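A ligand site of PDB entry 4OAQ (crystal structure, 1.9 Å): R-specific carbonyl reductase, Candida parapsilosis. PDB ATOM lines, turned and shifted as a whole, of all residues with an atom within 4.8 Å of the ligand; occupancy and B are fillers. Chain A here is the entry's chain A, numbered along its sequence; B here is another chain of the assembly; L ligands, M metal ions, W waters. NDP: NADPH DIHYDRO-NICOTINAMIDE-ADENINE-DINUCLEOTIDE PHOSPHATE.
Cys 48 touches the ligand (SG to C6N, 3.7 Å). His 53 touches the ligand. Trp 59 touches the ligand (CZ2 to O2D, 3.2 Å). SG of Cys 167 touches C5N of the ligand, 3.6 Å away. Thr 171 touches the ligand. Gly 193 touches the ligand (CA to O2B, 3.7 Å). O of Cys 256 touches C5D of the ligand, 3.3 Å away. Ala 257 touches the ligand (CA to O4B, 3.4 Å). C of Gly 259 touches N1A of the ligand (3.2 Å). Gly 282 touches the ligand (CA to O4D, 3.7 Å). Leu 308 touches the ligand. Of the 35 residues printed, 28 come within 4 Å of the ligand. The nearest printed residue that does not touch the ligand is Gly 262 (4.2 Å).
Water W3 bridges an oxygen (O1A) of the ligand (2.5 Å) and the side-chain hydroxyl of Ser 258 (2.6 Å). Water W7 bridges O1A of the ligand (2.5 Å) and O of Cys 348 (2.7 Å). Water W2 lies within hydrogen-bond range of an oxygen (O2A) of the ligand, the backbone carbonyl oxygen of Tyr 355 and the guanidinium group of Arg 356. Water W1 lies within hydrogen-bond range of the backbone carbonyl oxygen (O) of Tyr 355 and an oxygen (O2A) of the ligand.
The side-chain sulfur of Cys 48 sits close to the guanidinium group of Arg 356. NZ of Lys 221 sits at hydrogen-bond distance from O of Ile 194, 3.1 Å away. The side-chain sulfur of Cys 48 sits close to the backbone NH of Ser 50, 3.5 Å away. The indole nitrogen of Trp 59 lies within hydrogen-bond range of the backbone carbonyl oxygen of Leu 283. ND1 of His 53 sits close to O of Leu 283, 3.4 Å away. The backbone carbonyl oxygen of Pro 284 is in hydrogen-bond range of the indole nitrogen of Trp 59, 2.9 Å away. OG1 of Thr 171 is in hydrogen-bond range of O of Cys 167. The backbone NH of Gly 193 is in hydrogen-bond range of the backbone carbonyl oxygen of Phe 215.
OG of Ser 216 lies within hydrogen-bond range of O2X of the ligand (2.5 Å). NH1 of Arg 356 lies within salt-bridge range of O2N of the ligand, at 2.7 Å. An oxygen (O1X) of the ligand lies within salt-bridge range of the side-chain amino group (NZ) of Lys 221 (2.8 Å). O2D of the ligand is in hydrogen-bond range of OG of Ser 50, at 2.8 Å. An oxygen (O2A) of the ligand sits at hydrogen-bond distance from the backbone NH (N) of Gly 196, at 2.9 Å. An oxygen (O2X) of the ligand lies within hydrogen-bond range of the backbone NH (N) of Ile 194. The backbone carbonyl oxygen of Ile 194 is in hydrogen-bond range of an oxygen (O3B) of the ligand (3.5 Å). A nitrogen (N1A) of the ligand sits at hydrogen-bond distance from the backbone NH (N) of Asp 261 (2.9 Å). N of Tyr 49 is in hydrogen-bond range of O2N of the ligand (2.9 Å). The backbone NH (N) of Leu 197 is in hydrogen-bond range of an oxygen (O1N) of the ligand (2.9 Å). The backbone carbonyl oxygen of Val 281 sits close to a nitrogen (N7N) of the ligand (3.0 Å). N of Leu 309 lies within hydrogen-bond range of O7N of the ligand (3.0 Å). The backbone carbonyl oxygen (O) of Ser 307 sits at hydrogen-bond distance from a nitrogen (N7N) of the ligand (3.0 Å). N of Arg 217 is in hydrogen-bond range of O3X of the ligand. NE of Arg 217 is in salt-bridge range of O3X of the ligand (3.0 Å). The backbone NH of Ser 258 sits at hydrogen-bond distance from an oxygen (O4B) of the ligand. A nitrogen (N7A) of the ligand lies close to the side-chain hydroxyl (OG) of Ser 258, at 3.2 Å. An oxygen (O3D) of the ligand is in hydrogen-bond range of the backbone NH (N) of Leu 283 (3.1 Å). The backbone carbonyl oxygen (O) of Leu 283 sits at hydrogen-bond distance from an oxygen (O3D) of the ligand (3.2 Å). O3B of the ligand lies close to N of Gly 195 (3.4 Å). A nitrogen (N1A) of the ligand lies within hydrogen-bond range of the backbone NH of Ile 260 (3.4 Å).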
ATOM      1  N   CYS A  48      10.725   9.394  -6.002  1.00  0.00           N
ATOM      2  CA  CYS A  48      11.507  10.472  -6.602  1.00  0.00           C
ATOM      3  C   CYS A  48      10.978  10.728  -8.014  1.00  0.00           C
ATOM      4  O   CYS A  48      10.592   9.778  -8.685  1.00  0.00           O
ATOM      5  CB  CYS A  48      12.959  10.015  -6.665  1.00  0.00           C
ATOM      6  SG  CYS A  48      14.128  11.209  -7.388  1.00  0.00           S
ATOM      7  N   TYR A  49      10.978  11.979  -8.482  1.00  0.00           N
ATOM      8  CA  TYR A  49      10.475  12.218  -9.839  1.00  0.00           C
ATOM      9  C   TYR A  49      11.319  11.492 -10.884  1.00  0.00           C
ATOM     10  O   TYR A  49      10.865  11.216 -11.988  1.00  0.00           O
ATOM     11  CB  TYR A  49      10.349  13.697 -10.181  1.00  0.00           C
ATOM     12  CG  TYR A  49       9.260  13.932 -11.200  1.00  0.00           C
ATOM     13  CD1 TYR A  49       7.967  14.202 -10.816  1.00  0.00           C
ATOM     14  CD2 TYR A  49       9.544  13.864 -12.551  1.00  0.00           C
ATOM     15  CE1 TYR A  49       6.969  14.396 -11.744  1.00  0.00           C
ATOM     16  CE2 TYR A  49       8.563  14.057 -13.496  1.00  0.00           C
ATOM     17  CZ  TYR A  49       7.278  14.323 -13.082  1.00  0.00           C
ATOM     18  OH  TYR A  49       6.310  14.505 -14.026  1.00  0.00           O
ATOM     19  N   SER A  50      12.551  11.180 -10.505  1.00  0.00           N
ATOM     20  CA  SER A  50      13.416  10.332 -11.327  1.00  0.00           C
ATOM     21  C   SER A  50      12.760   8.992 -11.635  1.00  0.00           C
ATOM     22  O   SER A  50      12.945   8.432 -12.719  1.00  0.00           O
ATOM     23  CB  SER A  50      14.775  10.107 -10.649  1.00  0.00           C
ATOM     24  OG  SER A  50      15.534  11.313 -10.681  1.00  0.00           O
ATOM     25  N   HIS A  53      10.344   9.870 -14.543  1.00  0.00           N
ATOM     26  CA  HIS A  53      11.118  10.031 -15.766  1.00  0.00           C
ATOM     27  C   HIS A  53      11.634   8.694 -16.310  1.00  0.00           C
ATOM     28  O   HIS A  53      11.589   8.447 -17.520  1.00  0.00           O
ATOM     29  CB  HIS A  53      12.260  11.040 -15.566  1.00  0.00           C
ATOM     30  CG  HIS A  53      11.809  12.467 -15.666  1.00  0.00           C
ATOM     31  ND1 HIS A  53      12.348  13.475 -14.908  1.00  0.00           N
ATOM     32  CD2 HIS A  53      10.858  13.036 -16.435  1.00  0.00           C
ATOM     33  CE1 HIS A  53      11.757  14.616 -15.220  1.00  0.00           C
ATOM     34  NE2 HIS A  53      10.850  14.389 -16.141  1.00  0.00           N
ATOM     35  N   TRP A  59      13.777   9.808 -20.482  1.00  0.00           N
ATOM     36  CA  TRP A  59      15.207  10.016 -20.669  1.00  0.00           C
ATOM     37  C   TRP A  59      15.720   9.011 -21.684  1.00  0.00           C
ATOM     38  O   TRP A  59      16.362   9.384 -22.670  1.00  0.00           O
ATOM     39  CB  TRP A  59      15.961   9.834 -19.351  1.00  0.00           C
ATOM     40  CG  TRP A  59      15.745  10.888 -18.312  1.00  0.00           C
ATOM     41  CD1 TRP A  59      15.385  12.184 -18.511  1.00  0.00           C
ATOM     42  CD2 TRP A  59      15.881  10.717 -16.894  1.00  0.00           C
ATOM     43  NE1 TRP A  59      15.300  12.843 -17.300  1.00  0.00           N
ATOM     44  CE2 TRP A  59      15.588  11.949 -16.290  1.00  0.00           C
ATOM     45  CE3 TRP A  59      16.211   9.628 -16.082  1.00  0.00           C
ATOM     46  CZ2 TRP A  59      15.632  12.131 -14.902  1.00  0.00           C
ATOM     47  CZ3 TRP A  59      16.240   9.808 -14.714  1.00  0.00           C
ATOM     48  CH2 TRP A  59      15.962  11.045 -14.136  1.00  0.00           C
ATOM     49  N   CYS A 167      18.370  10.387  -1.346  1.00  0.00           N
ATOM     50  CA  CYS A 167      18.549  10.893  -2.713  1.00  0.00           C
ATOM     51  C   CYS A 167      18.270  12.387  -2.821  1.00  0.00           C
ATOM     52  O   CYS A 167      19.180  13.137  -3.142  1.00  0.00           O
ATOM     53  CB  CYS A 167      17.724  10.094  -3.727  1.00  0.00           C
ATOM     54  SG  CYS A 167      17.997  10.630  -5.461  1.00  0.00           S
ATOM     55  N   THR A 171      21.396  14.838  -2.841  1.00  0.00           N
ATOM     56  CA  THR A 171      21.517  15.471  -4.157  1.00  0.00           C
ATOM     57  C   THR A 171      21.519  16.981  -4.101  1.00  0.00           C
ATOM     58  O   THR A 171      22.222  17.630  -4.914  1.00  0.00           O
ATOM     59  CB  THR A 171      20.447  15.005  -5.152  1.00  0.00           C
ATOM     60  OG1 THR A 171      20.649  13.607  -5.414  1.00  0.00           O
ATOM     61  CG2 THR A 171      20.526  15.776  -6.475  1.00  0.00           C
ATOM     62  N   GLY A 193      12.316  25.529  -8.116  1.00  0.00           N
ATOM     63  CA  GLY A 193      11.517  24.327  -8.223  1.00  0.00           C
ATOM     64  C   GLY A 193      11.356  23.671  -6.871  1.00  0.00           C
ATOM     65  O   GLY A 193      12.172  22.835  -6.470  1.00  0.00           O
ATOM     66  N   ILE A 194      10.290  24.032  -6.160  1.00  0.00           N
ATOM     67  CA  ILE A 194      10.140  23.609  -4.771  1.00  0.00           C
ATOM     68  C   ILE A 194       9.368  22.291  -4.665  1.00  0.00           C
ATOM     69  O   ILE A 194       8.206  22.271  -4.253  1.00  0.00           O
ATOM     70  CB  ILE A 194       9.449  24.692  -3.928  1.00  0.00           C
ATOM     71  CG1 ILE A 194      10.034  26.081  -4.253  1.00  0.00           C
ATOM     72  CG2 ILE A 194       9.600  24.394  -2.464  1.00  0.00           C
ATOM     73  CD1 ILE A 194      11.550  26.181  -4.090  1.00  0.00           C
ATOM     74  N   GLY A 195      10.022  21.193  -5.056  1.00  0.00           N
ATOM     75  CA  GLY A 195       9.435  19.877  -4.963  1.00  0.00           C
ATOM     76  C   GLY A 195      10.174  19.062  -3.914  1.00  0.00           C
ATOM     77  O   GLY A 195      10.566  19.605  -2.884  1.00  0.00           O
ATOM     78  N   GLY A 196      10.330  17.759  -4.147  1.00  0.00           N
ATOM     79  CA  GLY A 196      11.114  16.921  -3.255  1.00  0.00           C
ATOM     80  C   GLY A 196      12.496  17.529  -3.015  1.00  0.00           C
ATOM     81  O   GLY A 196      12.830  17.899  -1.893  1.00  0.00           O
ATOM     82  N   LEU A 197      13.282  17.693  -4.077  1.00  0.00           N
ATOM     83  CA  LEU A 197      14.626  18.211  -3.908  1.00  0.00           C
ATOM     84  C   LEU A 197      14.601  19.618  -3.344  1.00  0.00           C
ATOM     85  O   LEU A 197      15.230  19.883  -2.313  1.00  0.00           O
ATOM     86  CB  LEU A 197      15.436  18.169  -5.215  1.00  0.00           C
ATOM     87  CG  LEU A 197      16.257  16.901  -5.479  1.00  0.00           C
ATOM     88  CD1 LEU A 197      15.338  15.722  -5.688  1.00  0.00           C
ATOM     89  CD2 LEU A 197      17.178  17.068  -6.688  1.00  0.00           C
ATOM     90  N   GLY A 198      13.866  20.503  -4.004  1.00  0.00           N
ATOM     91  CA  GLY A 198      13.931  21.915  -3.702  1.00  0.00           C
ATOM     92  C   GLY A 198      13.515  22.268  -2.287  1.00  0.00           C
ATOM     93  O   GLY A 198      14.098  23.182  -1.663  1.00  0.00           O
ATOM     94  N   PHE A 215      12.381  30.086  -5.706  1.00  0.00           N
ATOM     95  CA  PHE A 215      11.775  30.374  -7.004  1.00  0.00           C
ATOM     96  C   PHE A 215      10.799  29.281  -7.396  1.00  0.00           C
ATOM     97  O   PHE A 215      11.129  28.095  -7.377  1.00  0.00           O
ATOM     98  CB  PHE A 215      12.840  30.477  -8.094  1.00  0.00           C
ATOM     99  CG  PHE A 215      13.724  31.681  -7.978  1.00  0.00           C
ATOM    100  CD1 PHE A 215      13.372  32.882  -8.582  1.00  0.00           C
ATOM    101  CD2 PHE A 215      14.928  31.607  -7.288  1.00  0.00           C
ATOM    102  CE1 PHE A 215      14.199  33.990  -8.487  1.00  0.00           C
ATOM    103  CE2 PHE A 215      15.767  32.721  -7.182  1.00  0.00           C
ATOM    104  CZ  PHE A 215      15.393  33.922  -7.791  1.00  0.00           C
ATOM    105  N   SER A 216       9.592  29.697  -7.751  1.00  0.00           N
ATOM    106  CA  SER A 216       8.568  28.751  -8.168  1.00  0.00           C
ATOM    107  C   SER A 216       7.753  29.375  -9.280  1.00  0.00           C
ATOM    108  O   SER A 216       7.681  30.595  -9.377  1.00  0.00           O
ATOM    109  CB  SER A 216       7.672  28.394  -6.985  1.00  0.00           C
ATOM    110  OG  SER A 216       6.700  27.442  -7.363  1.00  0.00           O
ATOM    111  N   ARG A 217       7.137  28.553 -10.116  1.00  0.00           N
ATOM    112  CA  ARG A 217       6.316  29.075 -11.210  1.00  0.00           C
ATOM    113  C   ARG A 217       5.141  29.909 -10.684  1.00  0.00           C
ATOM    114  O   ARG A 217       4.720  30.861 -11.327  1.00  0.00           O
ATOM    115  CB  ARG A 217       5.809  27.911 -12.073  1.00  0.00           C
ATOM    116  CG  ARG A 217       6.939  27.162 -12.822  1.00  0.00           C
ATOM    117  CD  ARG A 217       6.447  25.857 -13.411  1.00  0.00           C
ATOM    118  NE  ARG A 217       5.936  24.965 -12.377  1.00  0.00           N
ATOM    119  CZ  ARG A 217       5.293  23.830 -12.617  1.00  0.00           C
ATOM    120  NH1 ARG A 217       5.068  23.453 -13.872  1.00  0.00           N
ATOM    121  NH2 ARG A 217       4.859  23.087 -11.610  1.00  0.00           N
ATOM    122  N   LYS A 221       2.976  27.820  -3.232  1.00  0.00           N
ATOM    123  CA  LYS A 221       3.851  27.226  -2.205  1.00  0.00           C
ATOM    124  C   LYS A 221       4.614  28.251  -1.357  1.00  0.00           C
ATOM    125  O   LYS A 221       5.549  27.897  -0.646  1.00  0.00           O
ATOM    126  CB  LYS A 221       4.841  26.232  -2.827  1.00  0.00           C
ATOM    127  CG  LYS A 221       4.203  25.051  -3.539  1.00  0.00           C
ATOM    128  CD  LYS A 221       5.255  24.251  -4.313  1.00  0.00           C
ATOM    129  CE  LYS A 221       4.622  23.097  -5.071  1.00  0.00           C
ATOM    130  NZ  LYS A 221       5.626  22.446  -5.975  1.00  0.00           N
ATOM    131  N   CYS A 256      16.202  22.765  -9.126  1.00  0.00           N
ATOM    132  CA  CYS A 256      15.624  21.500  -8.690  1.00  0.00           C
ATOM    133  C   CYS A 256      14.338  21.163  -9.441  1.00  0.00           C
ATOM    134  O   CYS A 256      13.612  20.268  -9.033  1.00  0.00           O
ATOM    135  CB  CYS A 256      15.313  21.549  -7.188  1.00  0.00           C
ATOM    136  SG  CYS A 256      16.761  21.860  -6.138  1.00  0.00           S
ATOM    137  N   ALA A 257      14.067  21.842 -10.536  1.00  0.00           N
ATOM    138  CA  ALA A 257      12.814  21.651 -11.232  1.00  0.00           C
ATOM    139  C   ALA A 257      12.807  20.360 -12.029  1.00  0.00           C
ATOM    140  O   ALA A 257      13.847  19.903 -12.513  1.00  0.00           O
ATOM    141  CB  ALA A 257      12.506  22.878 -12.142  1.00  0.00           C
ATOM    142  N   SER A 258      11.636  19.759 -12.204  1.00  0.00           N
ATOM    143  CA  SER A 258      11.553  18.519 -12.962  1.00  0.00           C
ATOM    144  C   SER A 258      11.512  18.733 -14.482  1.00  0.00           C
ATOM    145  O   SER A 258      11.590  17.772 -15.239  1.00  0.00           O
ATOM    146  CB  SER A 258      10.351  17.703 -12.511  1.00  0.00           C
ATOM    147  OG  SER A 258       9.182  18.507 -12.485  1.00  0.00           O
ATOM    148  N   GLY A 259      11.401  19.992 -14.922  1.00  0.00           N
ATOM    149  CA  GLY A 259      11.211  20.280 -16.332  1.00  0.00           C
ATOM    150  C   GLY A 259      11.761  21.639 -16.756  1.00  0.00           C
ATOM    151  O   GLY A 259      12.514  22.270 -16.007  1.00  0.00           O
ATOM    152  N   ILE A 260      11.394  22.080 -17.957  1.00  0.00           N
ATOM    153  CA  ILE A 260      11.872  23.354 -18.508  1.00  0.00           C
ATOM    154  C   ILE A 260      10.709  24.333 -18.627  1.00  0.00           C
ATOM    155  O   ILE A 260      10.902  25.468 -19.042  1.00  0.00           O
ATOM    156  CB  ILE A 260      12.475  23.195 -19.928  1.00  0.00           C
ATOM    157  CG1 ILE A 260      11.434  22.623 -20.894  1.00  0.00           C
ATOM    158  CG2 ILE A 260      13.744  22.345 -19.917  1.00  0.00           C
ATOM    159  CD1 ILE A 260      11.684  22.980 -22.373  1.00  0.00           C
ATOM    160  N   ASP A 261       9.516  23.875 -18.261  1.00  0.00           N
ATOM    161  CA  ASP A 261       8.263  24.601 -18.520  1.00  0.00           C
ATOM    162  C   ASP A 261       8.293  26.106 -18.287  1.00  0.00           C
ATOM    163  O   ASP A 261       8.210  26.883 -19.237  1.00  0.00           O
ATOM    164  CB  ASP A 261       7.079  23.919 -17.792  1.00  0.00           C
ATOM    165  CG  ASP A 261       5.837  24.800 -17.690  1.00  0.00           C
ATOM    166  OD1 ASP A 261       5.538  25.565 -18.636  1.00  0.00           O
ATOM    167  OD2 ASP A 261       5.148  24.703 -16.648  1.00  0.00           O
ATOM    168  N   GLY A 262       8.420  26.546 -17.037  1.00  0.00           N
ATOM    169  CA  GLY A 262       8.368  27.989 -16.810  1.00  0.00           C
ATOM    170  C   GLY A 262       9.720  28.633 -16.577  1.00  0.00           C
ATOM    171  O   GLY A 262       9.803  29.693 -15.949  1.00  0.00           O
ATOM    172  N   VAL A 281      20.452  20.332 -10.748  1.00  0.00           N
ATOM    173  CA  VAL A 281      20.299  18.945 -10.350  1.00  0.00           C
ATOM    174  C   VAL A 281      19.030  18.437 -10.996  1.00  0.00           C
ATOM    175  O   VAL A 281      18.865  17.233 -11.215  1.00  0.00           O
ATOM    176  CB  VAL A 281      20.281  18.714  -8.831  1.00  0.00           C
ATOM    177  CG1 VAL A 281      21.724  18.638  -8.302  1.00  0.00           C
ATOM    178  CG2 VAL A 281      19.513  19.809  -8.145  1.00  0.00           C
ATOM    179  N   GLY A 282      18.134  19.367 -11.333  1.00  0.00           N
ATOM    180  CA  GLY A 282      16.951  19.049 -12.119  1.00  0.00           C
ATOM    181  C   GLY A 282      17.329  18.456 -13.460  1.00  0.00           C
ATOM    182  O   GLY A 282      18.305  18.889 -14.087  1.00  0.00           O
ATOM    183  N   LEU A 283      16.555  17.476 -13.917  1.00  0.00           N
ATOM    184  CA  LEU A 283      16.849  16.745 -15.150  1.00  0.00           C
ATOM    185  C   LEU A 283      15.579  16.508 -15.971  1.00  0.00           C
ATOM    186  O   LEU A 283      14.893  15.500 -15.788  1.00  0.00           O
ATOM    187  CB  LEU A 283      17.498  15.396 -14.826  1.00  0.00           C
ATOM    188  CG  LEU A 283      18.799  15.393 -14.001  1.00  0.00           C
ATOM    189  CD1 LEU A 283      19.102  14.005 -13.421  1.00  0.00           C
ATOM    190  CD2 LEU A 283      19.972  15.877 -14.829  1.00  0.00           C
ATOM    191  N   PRO A 284      15.260  17.432 -16.897  1.00  0.00           N
ATOM    192  CA  PRO A 284      14.020  17.298 -17.673  1.00  0.00           C
ATOM    193  C   PRO A 284      14.069  16.075 -18.582  1.00  0.00           C
ATOM    194  O   PRO A 284      15.128  15.439 -18.661  1.00  0.00           O
ATOM    195  CB  PRO A 284      13.999  18.579 -18.507  1.00  0.00           C
ATOM    196  CG  PRO A 284      14.883  19.537 -17.745  1.00  0.00           C
ATOM    197  CD  PRO A 284      15.995  18.648 -17.280  1.00  0.00           C
ATOM    198  N   SER A 307      24.970  18.470 -11.555  1.00  0.00           N
ATOM    199  CA  SER A 307      25.625  17.772 -10.442  1.00  0.00           C
ATOM    200  C   SER A 307      24.839  16.482 -10.223  1.00  0.00           C
ATOM    201  O   SER A 307      23.646  16.456 -10.464  1.00  0.00           O
ATOM    202  CB  SER A 307      25.610  18.672  -9.197  1.00  0.00           C
ATOM    203  OG  SER A 307      26.022  17.982  -8.036  1.00  0.00           O
ATOM    204  N   LEU A 308      25.522  15.421  -9.793  1.00  0.00           N
ATOM    205  CA  LEU A 308      24.915  14.107  -9.644  1.00  0.00           C
ATOM    206  C   LEU A 308      25.061  13.608  -8.214  1.00  0.00           C
ATOM    207  O   LEU A 308      26.178  13.467  -7.708  1.00  0.00           O
ATOM    208  CB  LEU A 308      25.620  13.105 -10.589  1.00  0.00           C
ATOM    209  CG  LEU A 308      25.218  11.641 -10.610  1.00  0.00           C
ATOM    210  CD1 LEU A 308      23.772  11.420 -11.060  1.00  0.00           C
ATOM    211  CD2 LEU A 308      26.177  10.808 -11.465  1.00  0.00           C
ATOM    212  N   LEU A 309      23.934  13.380  -7.548  1.00  0.00           N
ATOM    213  CA  LEU A 309      23.951  12.760  -6.210  1.00  0.00           C
ATOM    214  C   LEU A 309      24.947  13.429  -5.261  1.00  0.00           C
ATOM    215  O   LEU A 309      25.054  14.640  -5.208  1.00  0.00           O
ATOM    216  CB  LEU A 309      24.280  11.281  -6.346  1.00  0.00           C
ATOM    217  CG  LEU A 309      23.278  10.597  -7.289  1.00  0.00           C
ATOM    218  CD1 LEU A 309      23.511   9.092  -7.313  1.00  0.00           C
ATOM    219  CD2 LEU A 309      21.850  10.935  -6.885  1.00  0.00           C
ATOM    220  N   CYS A 348       1.905  12.579  -7.929  1.00  0.00           N
ATOM    221  CA  CYS A 348       3.215  13.169  -8.099  1.00  0.00           C
ATOM    222  C   CYS A 348       3.341  13.815  -9.480  1.00  0.00           C
ATOM    223  O   CYS A 348       3.796  14.946  -9.594  1.00  0.00           O
ATOM    224  CB  CYS A 348       4.309  12.134  -7.870  1.00  0.00           C
ATOM    225  SG  CYS A 348       5.960  12.843  -7.887  1.00  0.00           S
ATOM    226  N   TYR A 355       5.732  17.203   0.536  1.00  0.00           N
ATOM    227  CA  TYR A 355       6.430  17.375  -0.739  1.00  0.00           C
ATOM    228  C   TYR A 355       7.028  16.078  -1.300  1.00  0.00           C
ATOM    229  O   TYR A 355       7.572  16.067  -2.399  1.00  0.00           O
ATOM    230  CB  TYR A 355       7.546  18.398  -0.547  1.00  0.00           C
ATOM    231  CG  TYR A 355       7.034  19.807  -0.461  1.00  0.00           C
ATOM    232  CD1 TYR A 355       6.969  20.615  -1.589  1.00  0.00           C
ATOM    233  CD2 TYR A 355       6.601  20.332   0.745  1.00  0.00           C
ATOM    234  CE1 TYR A 355       6.492  21.904  -1.507  1.00  0.00           C
ATOM    235  CE2 TYR A 355       6.123  21.621   0.827  1.00  0.00           C
ATOM    236  CZ  TYR A 355       6.075  22.405  -0.296  1.00  0.00           C
ATOM    237  OH  TYR A 355       5.595  23.673  -0.200  1.00  0.00           O
ATOM    238  N   ARG A 356       6.918  14.982  -0.550  1.00  0.00           N
ATOM    239  CA  ARG A 356       7.489  13.700  -0.977  1.00  0.00           C
ATOM    240  C   ARG A 356       6.605  12.538  -0.552  1.00  0.00           C
ATOM    241  O   ARG A 356       6.233  12.439   0.609  1.00  0.00           O
ATOM    242  CB  ARG A 356       8.870  13.510  -0.358  1.00  0.00           C
ATOM    243  CG  ARG A 356       9.992  13.608  -1.327  1.00  0.00           C
ATOM    244  CD  ARG A 356      10.114  12.355  -2.170  1.00  0.00           C
ATOM    245  NE  ARG A 356      11.414  12.279  -2.818  1.00  0.00           N
ATOM    246  CZ  ARG A 356      11.703  12.864  -3.978  1.00  0.00           C
ATOM    247  NH1 ARG A 356      10.783  13.559  -4.620  1.00  0.00           N
ATOM    248  NH2 ARG A 356      12.914  12.736  -4.508  1.00  0.00           N
ATOM    249  N   LEU B 298      26.293  16.146 -16.669  1.00  0.00           N
ATOM    250  CA  LEU B 298      25.961  15.332 -15.498  1.00  0.00           C
ATOM    251  C   LEU B 298      27.018  14.326 -15.018  1.00  0.00           C
ATOM    252  O   LEU B 298      27.312  14.264 -13.828  1.00  0.00           O
ATOM    253  CB  LEU B 298      24.656  14.607 -15.742  1.00  0.00           C
ATOM    254  CG  LEU B 298      24.121  13.847 -14.536  1.00  0.00           C
ATOM    255  CD1 LEU B 298      23.811  14.827 -13.424  1.00  0.00           C
ATOM    256  CD2 LEU B 298      22.882  13.085 -14.950  1.00  0.00           C
HETATM  257  PA  NDP L   1       9.175  16.952  -7.836  1.00  0.00           P
HETATM  258  O1A NDP L   1       8.078  16.626  -8.818  1.00  0.00           O
HETATM  259  O2A NDP L   1       9.046  16.525  -6.396  1.00  0.00           O
HETATM  260  O5B NDP L   1       9.494  18.520  -7.851  1.00  0.00           O
HETATM  261  C5B NDP L   1       9.745  19.144  -9.108  1.00  0.00           C
HETATM  262  C4B NDP L   1       9.352  20.601  -9.046  1.00  0.00           C
HETATM  263  O4B NDP L   1       9.572  21.184 -10.338  1.00  0.00           O
HETATM  264  C3B NDP L   1       7.880  20.802  -8.794  1.00  0.00           C
HETATM  265  O3B NDP L   1       7.625  20.840  -7.386  1.00  0.00           O
HETATM  266  C2B NDP L   1       7.581  22.127  -9.468  1.00  0.00           C
HETATM  267  O2B NDP L   1       8.068  23.189  -8.652  1.00  0.00           O
HETATM  268  C1B NDP L   1       8.519  22.104 -10.641  1.00  0.00           C
HETATM  269  N9A NDP L   1       7.964  21.605 -11.902  1.00  0.00           N
HETATM  270  C8A NDP L   1       7.045  20.636 -12.094  1.00  0.00           C
HETATM  271  N7A NDP L   1       6.842  20.436 -13.416  1.00  0.00           N
HETATM  272  C5A NDP L   1       7.639  21.270 -14.091  1.00  0.00           C
HETATM  273  C6A NDP L   1       7.918  21.565 -15.496  1.00  0.00           C
HETATM  274  N6A NDP L   1       7.246  20.904 -16.486  1.00  0.00           N
HETATM  275  N1A NDP L   1       8.848  22.526 -15.758  1.00  0.00           N
HETATM  276  C2A NDP L   1       9.496  23.182 -14.786  1.00  0.00           C
HETATM  277  N3A NDP L   1       9.287  22.957 -13.473  1.00  0.00           N
HETATM  278  C4A NDP L   1       8.387  22.031 -13.084  1.00  0.00           C
HETATM  279  O3  NDP L   1      10.503  16.286  -8.452  1.00  0.00           O
HETATM  280  PN  NDP L   1      11.798  15.859  -7.590  1.00  0.00           P
HETATM  281  O1N NDP L   1      12.086  16.989  -6.662  1.00  0.00           O
HETATM  282  O2N NDP L   1      11.611  14.467  -7.065  1.00  0.00           O
HETATM  283  O5D NDP L   1      12.884  15.798  -8.795  1.00  0.00           O
HETATM  284  C5D NDP L   1      13.255  17.027  -9.407  1.00  0.00           C
HETATM  285  C4D NDP L   1      14.248  16.797 -10.531  1.00  0.00           C
HETATM  286  O4D NDP L   1      15.513  16.396  -9.987  1.00  0.00           O
HETATM  287  C3D NDP L   1      13.774  15.683 -11.437  1.00  0.00           C
HETATM  288  O3D NDP L   1      14.062  16.087 -12.787  1.00  0.00           O
HETATM  289  C2D NDP L   1      14.638  14.519 -11.037  1.00  0.00           C
HETATM  290  O2D NDP L   1      14.810  13.611 -12.138  1.00  0.00           O
HETATM  291  C1D NDP L   1      15.933  15.221 -10.673  1.00  0.00           C
HETATM  292  N1N NDP L   1      16.866  14.484  -9.811  1.00  0.00           N
HETATM  293  C2N NDP L   1      18.184  14.622 -10.057  1.00  0.00           C
HETATM  294  C3N NDP L   1      19.136  13.957  -9.281  1.00  0.00           C
HETATM  295  C7N NDP L   1      20.576  14.151  -9.585  1.00  0.00           C
HETATM  296  O7N NDP L   1      21.409  13.358  -9.155  1.00  0.00           O
HETATM  297  N7N NDP L   1      20.906  15.248 -10.276  1.00  0.00           N
HETATM  298  C4N NDP L   1      18.713  13.186  -8.200  1.00  0.00           C
HETATM  299  C5N NDP L   1      17.347  13.079  -7.956  1.00  0.00           C
HETATM  300  C6N NDP L   1      16.436  13.750  -8.778  1.00  0.00           C
HETATM  301  P2B NDP L   1       7.262  24.598  -8.471  1.00  0.00           P
HETATM  302  O1X NDP L   1       5.835  24.138  -8.182  1.00  0.00           O
HETATM  303  O2X NDP L   1       7.933  25.289  -7.310  1.00  0.00           O
HETATM  304  O3X NDP L   1       7.425  25.334  -9.781  1.00  0.00           O
HETATM  305 ZN    ZN M   1      18.483   9.922 -10.627  1.00  0.00          ZN
HETATM  306  O   HOH W   1       6.806  17.538  -4.503  1.00  0.00           O
HETATM  307  O   HOH W   2       7.901  14.651  -4.806  1.00  0.00           O
HETATM  308  O   HOH W   3       7.327  17.480 -11.030  1.00  0.00           O
HETATM  309  O   HOH W   4      10.099  25.229 -11.723  1.00  0.00           O
HETATM  310  O   HOH W   5       6.406  18.514  -6.705  1.00  0.00           O
HETATM  311  O   HOH W   6      12.325  19.820  -6.419  1.00  0.00           O
HETATM  312  O   HOH W   7       5.571  16.633  -8.523  1.00  0.00           O
